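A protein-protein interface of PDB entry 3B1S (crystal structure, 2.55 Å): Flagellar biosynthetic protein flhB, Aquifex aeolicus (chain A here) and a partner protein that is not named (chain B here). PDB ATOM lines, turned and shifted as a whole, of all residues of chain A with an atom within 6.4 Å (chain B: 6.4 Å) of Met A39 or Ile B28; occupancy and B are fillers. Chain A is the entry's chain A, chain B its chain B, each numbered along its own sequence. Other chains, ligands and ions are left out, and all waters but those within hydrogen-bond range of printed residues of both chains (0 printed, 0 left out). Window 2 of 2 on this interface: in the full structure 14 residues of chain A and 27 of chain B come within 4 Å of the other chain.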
ATOM      1  N   LEU A  34      -8.033   3.787  13.461  1.00  0.00           N
ATOM      2  CA  LEU A  34      -9.249   4.352  14.003  1.00  0.00           C
ATOM      3  C   LEU A  34     -10.016   3.386  14.857  1.00  0.00           C
ATOM      4  O   LEU A  34     -10.619   3.758  15.834  1.00  0.00           O
ATOM      5  CB  LEU A  34     -10.127   4.872  12.891  1.00  0.00           C
ATOM      6  CG  LEU A  34      -9.699   6.121  12.167  1.00  0.00           C
ATOM      7  CD1 LEU A  34     -10.467   6.204  10.925  1.00  0.00           C
ATOM      8  CD2 LEU A  34     -10.005   7.259  12.995  1.00  0.00           C
ATOM      9  N   ALA A  35     -10.037   2.141  14.435  1.00  0.00           N
ATOM     10  CA  ALA A  35     -10.673   1.080  15.199  1.00  0.00           C
ATOM     11  C   ALA A  35     -10.004   1.038  16.592  1.00  0.00           C
ATOM     12  O   ALA A  35     -10.691   1.077  17.606  1.00  0.00           O
ATOM     13  CB  ALA A  35     -10.594  -0.251  14.461  1.00  0.00           C
ATOM     14  N   LYS A  36      -8.690   1.105  16.639  1.00  0.00           N
ATOM     15  CA  LYS A  36      -7.989   1.136  17.907  1.00  0.00           C
ATOM     16  C   LYS A  36      -8.277   2.337  18.798  1.00  0.00           C
ATOM     17  O   LYS A  36      -8.543   2.178  19.950  1.00  0.00           O
ATOM     18  CB  LYS A  36      -6.503   1.040  17.646  1.00  0.00           C
ATOM     19  CG  LYS A  36      -5.679   0.773  18.850  1.00  0.00           C
ATOM     20  CD  LYS A  36      -4.251   0.488  18.486  1.00  0.00           C
ATOM     21  CE  LYS A  36      -3.498   1.734  18.128  1.00  0.00           C
ATOM     22  NZ  LYS A  36      -3.523   2.725  19.208  1.00  0.00           N
ATOM     23  N   SER A  37      -8.286   3.545  18.295  1.00  0.00           N
ATOM     24  CA  SER A  37      -8.681   4.619  19.206  1.00  0.00           C
ATOM     25  C   SER A  37     -10.062   4.399  19.832  1.00  0.00           C
ATOM     26  O   SER A  37     -10.255   4.701  21.020  1.00  0.00           O
ATOM     27  CB  SER A  37      -8.605   5.987  18.543  1.00  0.00           C
ATOM     28  OG  SER A  37      -7.437   6.047  17.734  1.00  0.00           O
ATOM     29  N   ARG A  38     -11.019   3.870  19.057  1.00  0.00           N
ATOM     30  CA  ARG A  38     -12.360   3.615  19.589  1.00  0.00           C
ATOM     31  C   ARG A  38     -12.232   2.629  20.774  1.00  0.00           C
ATOM     32  O   ARG A  38     -12.680   2.904  21.909  1.00  0.00           O
ATOM     33  CB  ARG A  38     -13.308   3.069  18.505  1.00  0.00           C
ATOM     34  CG  ARG A  38     -13.314   1.501  18.427  1.00  0.00           C
ATOM     35  CD  ARG A  38     -13.980   0.935  17.209  1.00  0.00           C
ATOM     36  NE  ARG A  38     -15.346   1.433  17.010  1.00  0.00           N
ATOM     37  CZ  ARG A  38     -16.106   1.095  15.966  1.00  0.00           C
ATOM     38  NH1 ARG A  38     -17.341   1.574  15.863  1.00  0.00           N
ATOM     39  NH2 ARG A  38     -15.626   0.274  15.025  1.00  0.00           N
ATOM     40  N   MET A  39     -11.584   1.502  20.489  1.00  0.00           N
ATOM     41  CA  MET A  39     -11.434   0.442  21.438  1.00  0.00           C
ATOM     42  C   MET A  39     -10.784   0.885  22.784  1.00  0.00           C
ATOM     43  O   MET A  39     -11.342   0.594  23.854  1.00  0.00           O
ATOM     44  CB  MET A  39     -10.695  -0.692  20.783  1.00  0.00           C
ATOM     45  CG  MET A  39     -10.424  -1.777  21.717  1.00  0.00           C
ATOM     46  SD  MET A  39      -9.555  -3.151  20.951  1.00  0.00           S
ATOM     47  CE  MET A  39      -7.862  -2.652  21.237  1.00  0.00           C
ATOM     48  N   MET A  40      -9.652   1.608  22.726  1.00  0.00           N
ATOM     49  CA  MET A  40      -8.955   2.125  23.928  1.00  0.00           C
ATOM     50  C   MET A  40      -9.713   3.164  24.692  1.00  0.00           C
ATOM     51  O   MET A  40      -9.426   3.422  25.843  1.00  0.00           O
ATOM     52  CB  MET A  40      -7.606   2.724  23.584  1.00  0.00           C
ATOM     53  CG  MET A  40      -6.685   1.753  22.918  1.00  0.00           C
ATOM     54  SD  MET A  40      -6.292   0.390  24.014  1.00  0.00           S
ATOM     55  CE  MET A  40      -5.720  -0.776  22.798  1.00  0.00           C
ATOM     56  N   ALA A  41     -10.658   3.798  24.044  1.00  0.00           N
ATOM     57  CA  ALA A  41     -11.483   4.773  24.720  1.00  0.00           C
ATOM     58  C   ALA A  41     -12.646   4.058  25.457  1.00  0.00           C
ATOM     59  O   ALA A  41     -13.237   4.598  26.417  1.00  0.00           O
ATOM     60  CB  ALA A  41     -12.007   5.782  23.694  1.00  0.00           C
ATOM     61  N   GLU A  42     -12.976   2.847  24.994  1.00  0.00           N
ATOM     62  CA  GLU A  42     -14.070   2.070  25.576  1.00  0.00           C
ATOM     63  C   GLU A  42     -13.620   1.248  26.795  1.00  0.00           C
ATOM     64  O   GLU A  42     -14.452   0.632  27.483  1.00  0.00           O
ATOM     65  CB  GLU A  42     -14.723   1.167  24.510  1.00  0.00           C
ATOM     66  CG  GLU A  42     -15.820   1.856  23.687  1.00  0.00           C
ATOM     67  CD  GLU A  42     -16.956   2.470  24.551  1.00  0.00           C
ATOM     68  OE1 GLU A  42     -16.964   3.711  24.730  1.00  0.00           O
ATOM     69  OE2 GLU A  42     -17.835   1.722  25.049  1.00  0.00           O
ATOM     70  N   VAL A  43     -12.304   1.230  27.040  1.00  0.00           N
ATOM     71  CA  VAL A  43     -11.711   0.519  28.177  1.00  0.00           C
ATOM     72  C   VAL A  43     -12.083   1.112  29.551  1.00  0.00           C
ATOM     73  O   VAL A  43     -12.271   0.345  30.490  1.00  0.00           O
ATOM     74  CB  VAL A  43     -10.177   0.378  28.041  1.00  0.00           C
ATOM     75  CG1 VAL A  43      -9.578  -0.115  29.342  1.00  0.00           C
ATOM     76  CG2 VAL A  43      -9.813  -0.548  26.863  1.00  0.00           C
ATOM     77  N   PRO A  44     -12.354   2.388  29.647  1.00  0.00           N
ATOM     78  CA  PRO A  44     -12.700   2.986  30.921  1.00  0.00           C
ATOM     79  C   PRO A  44     -14.034   2.480  31.399  1.00  0.00           C
ATOM     80  O   PRO A  44     -14.503   2.820  32.458  1.00  0.00           O
ATOM     81  CB  PRO A  44     -12.763   4.448  30.570  1.00  0.00           C
ATOM     82  CG  PRO A  44     -11.672   4.583  29.664  1.00  0.00           C
ATOM     83  CD  PRO A  44     -11.624   3.347  28.830  1.00  0.00           C
ATOM     84  N   ALA B   5      -4.130  -9.211  26.485  1.00  0.00           N
ATOM     85  CA  ALA B   5      -5.180  -8.792  27.386  1.00  0.00           C
ATOM     86  C   ALA B   5      -6.556  -8.820  26.751  1.00  0.00           C
ATOM     87  O   ALA B   5      -6.676  -8.578  25.578  1.00  0.00           O
ATOM     88  CB  ALA B   5      -4.892  -7.419  27.843  1.00  0.00           C
ATOM     89  N   VAL B  21     -14.909  -5.476  25.407  1.00  0.00           N
ATOM     90  CA  VAL B  21     -14.771  -4.091  24.961  1.00  0.00           C
ATOM     91  C   VAL B  21     -13.418  -3.764  24.326  1.00  0.00           C
ATOM     92  O   VAL B  21     -13.279  -2.756  23.654  1.00  0.00           O
ATOM     93  CB  VAL B  21     -15.161  -3.048  26.040  1.00  0.00           C
ATOM     94  CG1 VAL B  21     -16.210  -3.612  26.951  1.00  0.00           C
ATOM     95  CG2 VAL B  21     -13.963  -2.538  26.830  1.00  0.00           C
ATOM     96  N   ALA B  22     -12.433  -4.629  24.536  1.00  0.00           N
ATOM     97  CA  ALA B  22     -11.115  -4.477  23.952  1.00  0.00           C
ATOM     98  C   ALA B  22     -10.423  -5.834  23.968  1.00  0.00           C
ATOM     99  O   ALA B  22     -10.706  -6.650  24.843  1.00  0.00           O
ATOM    100  CB  ALA B  22     -10.338  -3.497  24.742  1.00  0.00           C
ATOM    101  N   LYS B  23      -9.559  -6.094  22.981  1.00  0.00           N
ATOM    102  CA  LYS B  23      -8.561  -7.173  23.065  1.00  0.00           C
ATOM    103  C   LYS B  23      -7.199  -6.622  22.574  1.00  0.00           C
ATOM    104  O   LYS B  23      -7.184  -5.669  21.805  1.00  0.00           O
ATOM    105  CB  LYS B  23      -9.031  -8.437  22.335  1.00  0.00           C
ATOM    106  CG  LYS B  23      -9.047  -8.376  20.812  1.00  0.00           C
ATOM    107  CD  LYS B  23      -9.358  -9.746  20.220  1.00  0.00           C
ATOM    108  CE  LYS B  23      -9.667  -9.674  18.720  1.00  0.00           C
ATOM    109  NZ  LYS B  23      -9.856 -11.047  18.129  1.00  0.00           N
ATOM    110  N   GLY B  24      -6.077  -7.181  23.041  1.00  0.00           N
ATOM    111  CA  GLY B  24      -4.764  -6.549  22.835  1.00  0.00           C
ATOM    112  C   GLY B  24      -3.499  -7.391  22.948  1.00  0.00           C
ATOM    113  O   GLY B  24      -3.353  -8.197  23.879  1.00  0.00           O
ATOM    114  N   LYS B  25      -2.576  -7.204  21.998  1.00  0.00           N
ATOM    115  CA  LYS B  25      -1.241  -7.827  22.074  1.00  0.00           C
ATOM    116  C   LYS B  25      -0.184  -6.726  22.137  1.00  0.00           C
ATOM    117  O   LYS B  25      -0.423  -5.593  21.644  1.00  0.00           O
ATOM    118  CB  LYS B  25      -0.966  -8.727  20.867  1.00  0.00           C
ATOM    119  CG  LYS B  25      -1.841  -9.946  20.760  1.00  0.00           C
ATOM    120  CD  LYS B  25      -2.234 -10.142  19.286  1.00  0.00           C
ATOM    121  CE  LYS B  25      -3.267 -11.285  19.044  1.00  0.00           C
ATOM    122  NZ  LYS B  25      -4.129 -11.055  17.794  1.00  0.00           N
ATOM    123  N   GLY B  26       0.968  -7.044  22.737  1.00  0.00           N
ATOM    124  CA  GLY B  26       2.082  -6.096  22.767  1.00  0.00           C
ATOM    125  C   GLY B  26       1.765  -4.789  23.490  1.00  0.00           C
ATOM    126  O   GLY B  26       1.386  -4.804  24.675  1.00  0.00           O
ATOM    127  N   THR B  27       1.912  -3.650  22.812  1.00  0.00           N
ATOM    128  CA  THR B  27       1.782  -2.384  23.530  1.00  0.00           C
ATOM    129  C   THR B  27       0.318  -2.015  23.703  1.00  0.00           C
ATOM    130  O   THR B  27      -0.026  -1.217  24.591  1.00  0.00           O
ATOM    131  CB  THR B  27       2.536  -1.223  22.857  1.00  0.00           C
ATOM    132  OG1 THR B  27       2.160  -1.156  21.471  1.00  0.00           O
ATOM    133  CG2 THR B  27       4.073  -1.399  23.023  1.00  0.00           C
ATOM    134  N   ILE B  28      -0.531  -2.600  22.845  1.00  0.00           N
ATOM    135  CA  ILE B  28      -2.002  -2.485  22.935  1.00  0.00           C
ATOM    136  C   ILE B  28      -2.488  -3.123  24.255  1.00  0.00           C
ATOM    137  O   ILE B  28      -3.137  -2.474  25.067  1.00  0.00           O
ATOM    138  CB  ILE B  28      -2.713  -3.128  21.691  1.00  0.00           C
ATOM    139  CG1 ILE B  28      -2.212  -2.515  20.367  1.00  0.00           C
ATOM    140  CG2 ILE B  28      -4.231  -2.995  21.790  1.00  0.00           C
ATOM    141  CD1 ILE B  28      -2.694  -3.260  19.098  1.00  0.00           C
ATOM    142  N   ALA B  29      -2.147  -4.389  24.459  1.00  0.00           N
ATOM    143  CA  ALA B  29      -2.406  -5.044  25.720  1.00  0.00           C
ATOM    144  C   ALA B  29      -1.996  -4.175  26.918  1.00  0.00           C
ATOM    145  O   ALA B  29      -2.812  -3.944  27.841  1.00  0.00           O
ATOM    146  CB  ALA B  29      -1.690  -6.362  25.764  1.00  0.00           C
ATOM    147  N   GLN B  30      -0.733  -3.716  26.902  1.00  0.00           N
ATOM    148  CA  GLN B  30      -0.161  -2.916  27.983  1.00  0.00           C
ATOM    149  C   GLN B  30      -0.993  -1.665  28.216  1.00  0.00           C
ATOM    150  O   GLN B  30      -1.165  -1.243  29.359  1.00  0.00           O
ATOM    151  CB  GLN B  30       1.298  -2.535  27.681  1.00  0.00           C
ATOM    152  CG  GLN B  30       2.348  -3.546  28.145  1.00  0.00           C
ATOM    153  CD  GLN B  30       3.812  -3.012  28.130  1.00  0.00           C
ATOM    154  OE1 GLN B  30       4.221  -2.268  27.225  1.00  0.00           O
ATOM    155  NE2 GLN B  30       4.602  -3.419  29.131  1.00  0.00           N
ATOM    156  N   LYS B  31      -1.496  -1.073  27.139  1.00  0.00           N
ATOM    157  CA  LYS B  31      -2.328   0.131  27.194  1.00  0.00           C
ATOM    158  C   LYS B  31      -3.632  -0.104  27.884  1.00  0.00           C
ATOM    159  O   LYS B  31      -4.096   0.688  28.671  1.00  0.00           O
ATOM    160  CB  LYS B  31      -2.681   0.571  25.788  1.00  0.00           C
ATOM    161  CG  LYS B  31      -1.776   1.561  25.128  1.00  0.00           C
ATOM    162  CD  LYS B  31      -1.894   1.384  23.617  1.00  0.00           C
ATOM    163  CE  LYS B  31      -1.945   2.686  22.862  1.00  0.00           C
ATOM    164  NZ  LYS B  31      -2.559   2.521  21.537  1.00  0.00           N
ATOM    165  N   ILE B  32      -4.227  -1.245  27.598  1.00  0.00           N
ATOM    166  CA  ILE B  32      -5.456  -1.599  28.257  1.00  0.00           C
ATOM    167  C   ILE B  32      -5.249  -1.807  29.751  1.00  0.00           C
ATOM    168  O   ILE B  32      -5.830  -1.115  30.564  1.00  0.00           O
ATOM    169  CB  ILE B  32      -5.948  -2.897  27.639  1.00  0.00           C
ATOM    170  CG1 ILE B  32      -6.248  -2.678  26.163  1.00  0.00           C
ATOM    171  CG2 ILE B  32      -7.150  -3.396  28.342  1.00  0.00           C
ATOM    172  CD1 ILE B  32      -6.236  -3.907  25.326  1.00  0.00           C
ATOM    173  N   VAL B  33      -4.308  -2.652  30.115  1.00  0.00           N
ATOM    174  CA  VAL B  33      -3.921  -2.752  31.507  1.00  0.00           C
ATOM    175  C   VAL B  33      -3.741  -1.384  32.183  1.00  0.00           C
ATOM    176  O   VAL B  33      -4.211  -1.202  33.299  1.00  0.00           O
ATOM    177  CB  VAL B  33      -2.620  -3.559  31.653  1.00  0.00           C
ATOM    178  CG1 VAL B  33      -2.219  -3.649  33.098  1.00  0.00           C
ATOM    179  CG2 VAL B  33      -2.766  -4.956  31.013  1.00  0.00           C
ATOM    180  N   TYR B  54      -8.748 -15.131  23.222  1.00  0.00           N
ATOM    181  CA  TYR B  54      -8.381 -14.103  22.243  1.00  0.00           C
ATOM    182  C   TYR B  54      -8.916 -14.291  20.809  1.00  0.00           C
ATOM    183  O   TYR B  54      -9.640 -13.419  20.299  1.00  0.00           O
ATOM    184  CB  TYR B  54      -6.858 -13.914  22.205  1.00  0.00           C
ATOM    185  CG  TYR B  54      -6.463 -12.529  21.766  1.00  0.00           C
ATOM    186  CD1 TYR B  54      -5.839 -11.666  22.651  1.00  0.00           C
ATOM    187  CD2 TYR B  54      -6.752 -12.061  20.477  1.00  0.00           C
ATOM    188  CE1 TYR B  54      -5.493 -10.394  22.283  1.00  0.00           C
ATOM    189  CE2 TYR B  54      -6.405 -10.778  20.097  1.00  0.00           C
ATOM    190  CZ  TYR B  54      -5.778  -9.956  21.015  1.00  0.00           C
ATOM    191  OH  TYR B  54      -5.414  -8.683  20.692  1.00  0.00           O
ATOM    192  N   VAL B  59     -14.448  -7.571  19.432  1.00  0.00           N
ATOM    193  CA  VAL B  59     -14.799  -6.340  20.111  1.00  0.00           C
ATOM    194  C   VAL B  59     -16.228  -5.860  19.888  1.00  0.00           C
ATOM    195  O   VAL B  59     -16.634  -5.560  18.769  1.00  0.00           O
ATOM    196  CB  VAL B  59     -13.820  -5.243  19.738  1.00  0.00           C
ATOM    197  CG1 VAL B  59     -14.133  -3.953  20.504  1.00  0.00           C
ATOM    198  CG2 VAL B  59     -12.394  -5.726  20.007  1.00  0.00           C
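NZ of Lys A36 lies close to NZ of Lys B31 (2.5 Å). The backbone NH (N) of Lys B23 sits at hydrogen-bond distance from the side-chain sulfur (SD) of Met A39 (3.6 Å).
The side-chain amino group of Lys B23 sits at hydrogen-bond distance from the backbone carbonyl oxygen of Tyr B54 (3.2 Å).
O of Val B21 touches CG of Met A39, at 3.6 Å. CG of Met A39 touches CB of Ala B22, at 3.5 Å. Met A39 touches Ile B28 (CE to CG2, 3.7 Å). CG2 of Val B59 touches SD of Met A39, 3.9 Å away. Met A40 touches Ile B28. Met A40 touches Ile B32 (SD to CG1, 3.7 Å). Glu A42 touches Val B21. Ala B22 touches Val A43 (CB to CG2, 3.7 Å).
Of the printed residues of chain B, Lys A36 touches Lys B31. Met A39 touches just these residues of chain B: Val B21 (3.6 Å), Ala B22 (3.5 Å), Lys B23 (3.1 Å), Ile B28 (3.7 Å) and Val B59 (3.9 Å). Of the printed residues of chain B, Val A43 touches Ala B22 (3.7 Å). Of the printed residues of chain A, Val B21 touches Met A39 (3.6 Å) and Glu A42 (3.3 Å). Printed residues of chain A within 4 Å of Ala B22: Met A39 and Val A43. Of chain A, only Met A39 (3.7 Å) and Met A40 (2.9 Å) come within 4 Å of Ile B28. The nearest residue of chain A that does not touch Ile B28 is Lys A36 (4.1 Å). The nearest printed residue of chain B that does not touch Met A40 is Lys B31 (4.03 Å).
Printed residues of chain B that touch a printed residue of chain A: Val B21, Ala B22, Lys B23, Ile B28, Lys B31, Ile B32 and Val B59. Hydrophobic or aromatic side chains of chain B that line the printed part of chain A: Val B21, Ala B22, Ile B28, Ile B32 and Val B59. Printed residues of chain A that touch a printed residue of chain B: Lys A36, Met A39, Met A40, Glu A42 and Val A43. Hydrophobic or aromatic side chains of chain A within 4 Å of the printed part of chain B: Met A39, Met A40 and Val A43. Among the printed residues, no Asp or Glu carboxylate lies within 4 Å of a Lys or Arg side-chain nitrogen of the other chain.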
